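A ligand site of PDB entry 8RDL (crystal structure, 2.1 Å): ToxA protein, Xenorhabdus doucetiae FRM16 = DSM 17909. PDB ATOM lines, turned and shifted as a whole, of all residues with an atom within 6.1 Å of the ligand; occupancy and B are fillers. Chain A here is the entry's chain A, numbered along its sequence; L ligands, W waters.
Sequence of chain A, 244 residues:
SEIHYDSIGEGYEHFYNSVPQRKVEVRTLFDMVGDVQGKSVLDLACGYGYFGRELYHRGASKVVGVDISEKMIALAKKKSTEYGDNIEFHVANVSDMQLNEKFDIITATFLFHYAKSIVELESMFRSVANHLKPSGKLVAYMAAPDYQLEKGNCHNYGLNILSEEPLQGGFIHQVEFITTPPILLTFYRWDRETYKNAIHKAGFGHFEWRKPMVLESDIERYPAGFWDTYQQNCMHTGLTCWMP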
ATOM      1  N   LEU A  29      -7.537  27.820  23.574  1.00  0.00           N
ATOM      2  CA  LEU A  29      -6.135  27.429  23.291  1.00  0.00           C
ATOM      3  C   LEU A  29      -5.433  27.111  24.617  1.00  0.00           C
ATOM      4  O   LEU A  29      -4.858  26.016  24.718  1.00  0.00           O
ATOM      5  CB  LEU A  29      -5.456  28.566  22.519  1.00  0.00           C
ATOM      6  CG  LEU A  29      -4.081  28.255  21.933  1.00  0.00           C
ATOM      7  CD1 LEU A  29      -4.026  26.874  21.308  1.00  0.00           C
ATOM      8  CD2 LEU A  29      -3.688  29.309  20.911  1.00  0.00           C
ATOM      9  N   ASP A  43       6.754  23.751  21.048  1.00  0.00           N
ATOM     10  CA  ASP A  43       5.956  24.719  20.245  1.00  0.00           C
ATOM     11  C   ASP A  43       6.407  24.604  18.785  1.00  0.00           C
ATOM     12  O   ASP A  43       7.534  25.030  18.491  1.00  0.00           O
ATOM     13  CB  ASP A  43       6.111  26.127  20.822  1.00  0.00           C
ATOM     14  CG  ASP A  43       5.193  27.172  20.227  1.00  0.00           C
ATOM     15  OD1 ASP A  43       4.183  26.800  19.603  1.00  0.00           O
ATOM     16  OD2 ASP A  43       5.490  28.363  20.416  1.00  0.00           O
ATOM     17  N   LEU A  44       5.580  23.989  17.937  1.00  0.00           N
ATOM     18  CA  LEU A  44       5.822  23.820  16.481  1.00  0.00           C
ATOM     19  C   LEU A  44       5.228  25.019  15.733  1.00  0.00           C
ATOM     20  O   LEU A  44       4.198  25.541  16.188  1.00  0.00           O
ATOM     21  CB  LEU A  44       5.209  22.512  15.989  1.00  0.00           C
ATOM     22  CG  LEU A  44       5.656  21.250  16.729  1.00  0.00           C
ATOM     23  CD1 LEU A  44       5.049  20.008  16.094  1.00  0.00           C
ATOM     24  CD2 LEU A  44       7.185  21.155  16.739  1.00  0.00           C
ATOM     25  N   ALA A  45       5.862  25.431  14.639  1.00  0.00           N
ATOM     26  CA  ALA A  45       5.502  26.651  13.880  1.00  0.00           C
ATOM     27  C   ALA A  45       5.482  27.830  14.868  1.00  0.00           C
ATOM     28  O   ALA A  45       4.529  28.637  14.817  1.00  0.00           O
ATOM     29  CB  ALA A  45       4.174  26.442  13.198  1.00  0.00           C
ATOM     30  N   CYS A  46       6.497  27.913  15.725  1.00  0.00           N
ATOM     31  CA  CYS A  46       6.570  28.800  16.912  1.00  0.00           C
ATOM     32  C   CYS A  46       6.673  30.283  16.506  1.00  0.00           C
ATOM     33  O   CYS A  46       6.381  31.139  17.352  1.00  0.00           O
ATOM     34  CB  CYS A  46       7.731  28.424  17.822  1.00  0.00           C
ATOM     35  SG  CYS A  46       9.363  28.497  17.030  1.00  0.00           S
ATOM     36  N   GLY A  47       7.060  30.584  15.264  1.00  0.00           N
ATOM     37  CA  GLY A  47       7.408  31.957  14.857  1.00  0.00           C
ATOM     38  C   GLY A  47       8.534  32.489  15.729  1.00  0.00           C
ATOM     39  O   GLY A  47       9.556  31.783  15.864  1.00  0.00           O
ATOM     40  N   TYR A  50       6.117  33.337  20.569  1.00  0.00           N
ATOM     41  CA  TYR A  50       5.074  34.028  21.377  1.00  0.00           C
ATOM     42  C   TYR A  50       4.422  33.037  22.353  1.00  0.00           C
ATOM     43  O   TYR A  50       4.376  33.319  23.575  1.00  0.00           O
ATOM     44  CB  TYR A  50       4.015  34.653  20.473  1.00  0.00           C
ATOM     45  CG  TYR A  50       2.805  35.173  21.205  1.00  0.00           C
ATOM     46  CD1 TYR A  50       1.653  34.391  21.325  1.00  0.00           C
ATOM     47  CD2 TYR A  50       2.803  36.426  21.788  1.00  0.00           C
ATOM     48  CE1 TYR A  50       0.541  34.856  22.012  1.00  0.00           C
ATOM     49  CE2 TYR A  50       1.693  36.903  22.481  1.00  0.00           C
ATOM     50  CZ  TYR A  50       0.562  36.110  22.585  1.00  0.00           C
ATOM     51  OH  TYR A  50      -0.536  36.578  23.260  1.00  0.00           O
ATOM     52  N   PHE A  51       3.916  31.915  21.818  1.00  0.00           N
ATOM     53  CA  PHE A  51       3.036  30.968  22.542  1.00  0.00           C
ATOM     54  C   PHE A  51       3.839  30.140  23.549  1.00  0.00           C
ATOM     55  O   PHE A  51       3.428  30.058  24.713  1.00  0.00           O
ATOM     56  CB  PHE A  51       2.260  30.090  21.555  1.00  0.00           C
ATOM     57  CG  PHE A  51       1.116  29.341  22.180  1.00  0.00           C
ATOM     58  CD1 PHE A  51       0.191  29.996  22.979  1.00  0.00           C
ATOM     59  CD2 PHE A  51       0.979  27.973  21.987  1.00  0.00           C
ATOM     60  CE1 PHE A  51      -0.852  29.305  23.567  1.00  0.00           C
ATOM     61  CE2 PHE A  51      -0.075  27.289  22.583  1.00  0.00           C
ATOM     62  CZ  PHE A  51      -0.986  27.947  23.371  1.00  0.00           C
ATOM     63  N   VAL A  66      10.206  25.199  17.463  1.00  0.00           N
ATOM     64  CA  VAL A  66      10.628  24.737  16.117  1.00  0.00           C
ATOM     65  C   VAL A  66       9.857  25.540  15.068  1.00  0.00           C
ATOM     66  O   VAL A  66       8.622  25.662  15.190  1.00  0.00           O
ATOM     67  CB  VAL A  66      10.413  23.216  15.957  1.00  0.00           C
ATOM     68  CG1 VAL A  66      10.594  22.759  14.513  1.00  0.00           C
ATOM     69  CG2 VAL A  66      11.319  22.419  16.884  1.00  0.00           C
ATOM     70  N   ASP A  67      10.571  26.068  14.076  1.00  0.00           N
ATOM     71  CA  ASP A  67       9.995  26.759  12.893  1.00  0.00           C
ATOM     72  C   ASP A  67      10.899  26.484  11.684  1.00  0.00           C
ATOM     73  O   ASP A  67      12.122  26.351  11.878  1.00  0.00           O
ATOM     74  CB  ASP A  67       9.817  28.256  13.150  1.00  0.00           C
ATOM     75  CG  ASP A  67       8.795  28.903  12.240  1.00  0.00           C
ATOM     76  OD1 ASP A  67       9.093  29.056  11.039  1.00  0.00           O
ATOM     77  OD2 ASP A  67       7.701  29.245  12.729  1.00  0.00           O
ATOM     78  N   ILE A  68      10.306  26.382  10.490  1.00  0.00           N
ATOM     79  CA  ILE A  68      11.014  26.097   9.204  1.00  0.00           C
ATOM     80  C   ILE A  68      11.779  27.355   8.757  1.00  0.00           C
ATOM     81  O   ILE A  68      12.736  27.189   7.994  1.00  0.00           O
ATOM     82  CB  ILE A  68      10.019  25.599   8.135  1.00  0.00           C
ATOM     83  CG1 ILE A  68      10.732  24.891   6.984  1.00  0.00           C
ATOM     84  CG2 ILE A  68       9.135  26.737   7.635  1.00  0.00           C
ATOM     85  CD1 ILE A  68       9.809  24.209   6.004  1.00  0.00           C
ATOM     86  N   SER A  69      11.363  28.545   9.202  1.00  0.00           N
ATOM     87  CA  SER A  69      11.921  29.863   8.768  1.00  0.00           C
ATOM     88  C   SER A  69      13.147  30.241   9.591  1.00  0.00           C
ATOM     89  O   SER A  69      13.018  30.424  10.813  1.00  0.00           O
ATOM     90  CB  SER A  69      10.878  30.946   8.860  1.00  0.00           C
ATOM     91  OG  SER A  69      11.463  32.223   8.661  1.00  0.00           O
ATOM     92  N   MET A  72      12.425  33.568  11.323  1.00  0.00           N
ATOM     93  CA  MET A  72      11.555  33.503  12.530  1.00  0.00           C
ATOM     94  C   MET A  72      12.367  33.026  13.743  1.00  0.00           C
ATOM     95  O   MET A  72      12.173  33.597  14.839  1.00  0.00           O
ATOM     96  CB  MET A  72      10.366  32.566  12.298  1.00  0.00           C
ATOM     97  CG  MET A  72       9.378  33.103  11.294  1.00  0.00           C
ATOM     98  SD  MET A  72       8.785  34.770  11.709  1.00  0.00           S
ATOM     99  CE  MET A  72       7.476  34.941  10.500  1.00  0.00           C
ATOM    100  N   ALA A  92      13.755  23.765  11.716  1.00  0.00           N
ATOM    101  CA  ALA A  92      13.390  22.418  11.238  1.00  0.00           C
ATOM    102  C   ALA A  92      12.012  22.423  10.565  1.00  0.00           C
ATOM    103  O   ALA A  92      11.137  23.214  10.969  1.00  0.00           O
ATOM    104  CB  ALA A  92      13.437  21.437  12.385  1.00  0.00           C
ATOM    105  N   ASN A  93      11.857  21.578   9.549  1.00  0.00           N
ATOM    106  CA  ASN A  93      10.564  21.164   8.962  1.00  0.00           C
ATOM    107  C   ASN A  93       9.968  20.095   9.887  1.00  0.00           C
ATOM    108  O   ASN A  93      10.681  19.106  10.163  1.00  0.00           O
ATOM    109  CB  ASN A  93      10.744  20.656   7.528  1.00  0.00           C
ATOM    110  CG  ASN A  93       9.439  20.421   6.793  1.00  0.00           C
ATOM    111  OD1 ASN A  93       8.412  20.132   7.407  1.00  0.00           O
ATOM    112  ND2 ASN A  93       9.471  20.549   5.483  1.00  0.00           N
ATOM    113  N   VAL A  94       8.730  20.283  10.361  1.00  0.00           N
ATOM    114  CA  VAL A  94       8.064  19.356  11.321  1.00  0.00           C
ATOM    115  C   VAL A  94       8.044  17.939  10.726  1.00  0.00           C
ATOM    116  O   VAL A  94       8.262  16.995  11.505  1.00  0.00           O
ATOM    117  CB  VAL A  94       6.663  19.847  11.725  1.00  0.00           C
ATOM    118  CG1 VAL A  94       5.859  18.767  12.444  1.00  0.00           C
ATOM    119  CG2 VAL A  94       6.722  21.108  12.579  1.00  0.00           C
ATOM    120  N   SER A  95       7.826  17.803   9.414  1.00  0.00           N
ATOM    121  CA  SER A  95       7.676  16.504   8.686  1.00  0.00           C
ATOM    122  C   SER A  95       8.893  15.594   8.885  1.00  0.00           C
ATOM    123  O   SER A  95       8.707  14.366   8.795  1.00  0.00           O
ATOM    124  CB  SER A  95       7.422  16.723   7.210  1.00  0.00           C
ATOM    125  OG  SER A  95       6.355  17.640   6.988  1.00  0.00           O
ATOM    126  N   ALA A 108       0.747  23.097  18.052  1.00  0.00           N
ATOM    127  CA  ALA A 108       0.889  23.236  16.585  1.00  0.00           C
ATOM    128  C   ALA A 108      -0.239  24.137  16.073  1.00  0.00           C
ATOM    129  O   ALA A 108      -1.157  23.612  15.398  1.00  0.00           O
ATOM    130  CB  ALA A 108       0.879  21.874  15.937  1.00  0.00           C
ATOM    131  N   THR A 109      -0.180  25.431  16.397  1.00  0.00           N
ATOM    132  CA  THR A 109      -1.188  26.440  15.992  1.00  0.00           C
ATOM    133  C   THR A 109      -0.844  26.956  14.586  1.00  0.00           C
ATOM    134  O   THR A 109       0.238  27.560  14.413  1.00  0.00           O
ATOM    135  CB  THR A 109      -1.305  27.525  17.074  1.00  0.00           C
ATOM    136  OG1 THR A 109      -0.020  28.071  17.360  1.00  0.00           O
ATOM    137  CG2 THR A 109      -1.881  26.993  18.360  1.00  0.00           C
ATOM    138  N   PHE A 110      -1.738  26.678  13.621  1.00  0.00           N
ATOM    139  CA  PHE A 110      -1.667  27.106  12.196  1.00  0.00           C
ATOM    140  C   PHE A 110      -0.445  26.517  11.492  1.00  0.00           C
ATOM    141  O   PHE A 110       0.143  27.198  10.644  1.00  0.00           O
ATOM    142  CB  PHE A 110      -1.646  28.634  12.090  1.00  0.00           C
ATOM    143  CG  PHE A 110      -2.659  29.320  12.966  1.00  0.00           C
ATOM    144  CD1 PHE A 110      -4.022  29.182  12.717  1.00  0.00           C
ATOM    145  CD2 PHE A 110      -2.260  30.064  14.063  1.00  0.00           C
ATOM    146  CE1 PHE A 110      -4.952  29.781  13.538  1.00  0.00           C
ATOM    147  CE2 PHE A 110      -3.197  30.674  14.879  1.00  0.00           C
ATOM    148  CZ  PHE A 110      -4.537  30.537  14.620  1.00  0.00           C
ATOM    149  N   LEU A 111      -0.094  25.277  11.838  1.00  0.00           N
ATOM    150  CA  LEU A 111       0.971  24.498  11.164  1.00  0.00           C
ATOM    151  C   LEU A 111       0.353  23.702  10.006  1.00  0.00           C
ATOM    152  O   LEU A 111       0.884  23.750   8.897  1.00  0.00           O
ATOM    153  CB  LEU A 111       1.625  23.547  12.175  1.00  0.00           C
ATOM    154  CG  LEU A 111       2.508  22.451  11.580  1.00  0.00           C
ATOM    155  CD1 LEU A 111       3.675  23.039  10.805  1.00  0.00           C
ATOM    156  CD2 LEU A 111       3.009  21.511  12.660  1.00  0.00           C
ATOM    157  N   TYR A 114      -0.326  24.400   6.214  1.00  0.00           N
ATOM    158  CA  TYR A 114       0.868  24.491   5.336  1.00  0.00           C
ATOM    159  C   TYR A 114       1.194  23.127   4.715  1.00  0.00           C
ATOM    160  O   TYR A 114       2.036  23.094   3.815  1.00  0.00           O
ATOM    161  CB  TYR A 114       2.093  25.009   6.092  1.00  0.00           C
ATOM    162  CG  TYR A 114       2.071  26.472   6.428  1.00  0.00           C
ATOM    163  CD1 TYR A 114       2.806  27.394   5.680  1.00  0.00           C
ATOM    164  CD2 TYR A 114       1.343  26.949   7.507  1.00  0.00           C
ATOM    165  CE1 TYR A 114       2.805  28.745   5.998  1.00  0.00           C
ATOM    166  CE2 TYR A 114       1.330  28.297   7.836  1.00  0.00           C
ATOM    167  CZ  TYR A 114       2.061  29.193   7.076  1.00  0.00           C
ATOM    168  OH  TYR A 114       2.027  30.510   7.426  1.00  0.00           O
ATOM    169  N   GLU A 120       2.143  14.717   3.297  1.00  0.00           N
ATOM    170  CA  GLU A 120       2.849  15.710   4.159  1.00  0.00           C
ATOM    171  C   GLU A 120       2.077  15.857   5.473  1.00  0.00           C
ATOM    172  O   GLU A 120       2.721  15.854   6.539  1.00  0.00           O
ATOM    173  CB  GLU A 120       3.030  17.054   3.469  1.00  0.00           C
ATOM    174  CG  GLU A 120       4.003  17.942   4.210  1.00  0.00           C
ATOM    175  CD  GLU A 120       4.213  19.326   3.647  1.00  0.00           C
ATOM    176  OE1 GLU A 120       5.030  20.066   4.207  1.00  0.00           O
ATOM    177  OE2 GLU A 120       3.543  19.664   2.661  1.00  0.00           O
ATOM    178  N   MET A 124       3.608  15.012   9.187  1.00  0.00           N
ATOM    179  CA  MET A 124       3.608  15.993  10.308  1.00  0.00           C
ATOM    180  C   MET A 124       3.030  15.332  11.570  1.00  0.00           C
ATOM    181  O   MET A 124       3.676  15.434  12.627  1.00  0.00           O
ATOM    182  CB  MET A 124       2.781  17.227   9.959  1.00  0.00           C
ATOM    183  CG  MET A 124       3.465  18.179   8.990  1.00  0.00           C
ATOM    184  SD  MET A 124       2.442  19.644   8.738  1.00  0.00           S
ATOM    185  CE  MET A 124       3.468  20.558   7.586  1.00  0.00           C
HETATM  186  N1  LIG L   1       2.246  28.998  16.098  1.00  0.00           N
HETATM  187  C1  LIG L   1       2.165  30.416  15.595  1.00  0.00           C
HETATM  188  C2  LIG L   1       2.017  30.456  14.068  1.00  0.00           C
HETATM  189  C3  LIG L   1       3.000  31.380  13.383  1.00  0.00           C
HETATM  190  S1  LIG L   1       2.663  31.569  11.620  1.00  0.00           S
HETATM  191  C4  LIG L   1       0.958  31.129  16.229  1.00  0.00           C
HETATM  192  O1  LIG L   1      -0.013  30.492  16.630  1.00  0.00           O
HETATM  193  O2  LIG L   1       0.931  32.347  16.349  1.00  0.00           O
HETATM  194  C5  LIG L   1       3.005  29.938  10.945  1.00  0.00           C
HETATM  195  C6  LIG L   1       4.452  29.533  11.070  1.00  0.00           C
HETATM  196  O3  LIG L   1       4.597  28.167  10.609  1.00  0.00           O
HETATM  197  C7  LIG L   1       5.438  30.358  10.241  1.00  0.00           C
HETATM  198  O4  LIG L   1       6.387  30.979  11.106  1.00  0.00           O
HETATM  199  C8  LIG L   1       6.100  29.328   9.310  1.00  0.00           C
HETATM  200  O5  LIG L   1       7.474  29.569   9.110  1.00  0.00           O
HETATM  201  C9  LIG L   1       5.884  28.035  10.085  1.00  0.00           C
HETATM  202  N2  LIG L   1       5.924  26.807   9.301  1.00  0.00           N
HETATM  203  C10 LIG L   1       5.309  26.583   8.089  1.00  0.00           C
HETATM  204  N3  LIG L   1       5.507  25.380   7.632  1.00  0.00           N
HETATM  205  C11 LIG L   1       6.289  24.763   8.597  1.00  0.00           C
HETATM  206  C12 LIG L   1       6.833  23.464   8.691  1.00  0.00           C
HETATM  207  N4  LIG L   1       6.663  22.516   7.769  1.00  0.00           N
HETATM  208  N5  LIG L   1       7.567  23.175   9.792  1.00  0.00           N
HETATM  209  C13 LIG L   1       7.738  24.123  10.713  1.00  0.00           C
HETATM  210  N6  LIG L   1       7.279  25.375  10.732  1.00  0.00           N
HETATM  211  C14 LIG L   1       6.548  25.631   9.633  1.00  0.00           C
HETATM  212  O   HOH W   1       3.300  33.402  16.532  1.00  0.00           O
HETATM  213  O   HOH W   2       2.197  26.330  17.990  1.00  0.00           O
HETATM  214  O   HOH W   3       5.035  22.462   5.114  1.00  0.00           O
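The backbone carbonyl oxygen (O) of Asp 67 lies within hydrogen-bond range of the backbone NH (N) of Ala 92 (3.1 Å). N of Ser 69 lies within hydrogen-bond range of OD1 of Asp 67, at 3.0 Å. The side-chain carboxylate (OD2) of Asp 67 is in hydrogen-bond range of the backbone NH (N) of Gly 47 (2.9 Å). The side-chain carboxylate of Asp 67 is in hydrogen-bond range of the backbone NH of Cys 46 (3.5 Å). O of Val 66 lies within hydrogen-bond range of N of Ala 45 (2.8 Å). The backbone NH (N) of Ser 95 is in hydrogen-bond range of the side-chain amide oxygen (OD1) of Asn 93, at 3.1 Å. The backbone carbonyl oxygen of Ala 92 is in hydrogen-bond range of the backbone NH of Ile 68 (3.3 Å). The side-chain hydroxyl (OG) of Ser 69 lies within hydrogen-bond range of the backbone NH (N) of Met 72 (3.1 Å).
The backbone carbonyl oxygen of Thr 109 is in hydrogen-bond range of a nitrogen (N1) of the ligand. O1 of the ligand lies within hydrogen-bond range of OG1 of Thr 109, at 2.5 Å. An oxygen (O5) of the ligand lies within hydrogen-bond range of the side-chain carboxylate (OD1) of Asp 67 (2.6 Å). The backbone carbonyl oxygen of Ala 45 sits at hydrogen-bond distance from a nitrogen (N1) of the ligand, 2.6 Å away. A nitrogen (N4) of the ligand lies within hydrogen-bond range of the side-chain amide oxygen of Asn 93 (3.0 Å). The backbone NH (N) of Val 94 sits at hydrogen-bond distance from a nitrogen (N5) of the ligand, 3.2 Å away. The backbone NH (N) of Ile 68 sits at hydrogen-bond distance from a nitrogen (N6) of the ligand (3.2 Å).
Water W3 lies within hydrogen-bond range of OE1 of Glu 120 (2.6 Å), N4 of the ligand (3.1 Å) and O of Tyr 114 (3.3 Å). Water W2 lies within hydrogen-bond range of the side-chain carboxylate of Asp 43 (2.6 Å), the backbone carbonyl oxygen of Leu 44 (2.8 Å), the side-chain hydroxyl of Thr 109 (2.9 Å) and a nitrogen (N1) of the ligand (3.3 Å).
Residues that only touch the ligand: Leu 44 (3.97 Å), Ser 69 (3.7 Å), Met 72 (3.7 Å), Ala 92 (3.5 Å), Phe 110 (3.4 Å), Leu 111 (3.8 Å), Tyr 114 (3.6 Å) and Met 124 (3.8 Å). 14 residues have an atom within 4 Å of the ligand: Leu 44, Ala 45, Asp 67, Ile 68, Ser 69, Met 72, Ala 92, Asn 93, Val 94, Thr 109, Phe 110, Leu 111, Tyr 114 and Met 124. The nearest printed residue that does not touch the ligand is Gly 47 (4.01 Å).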
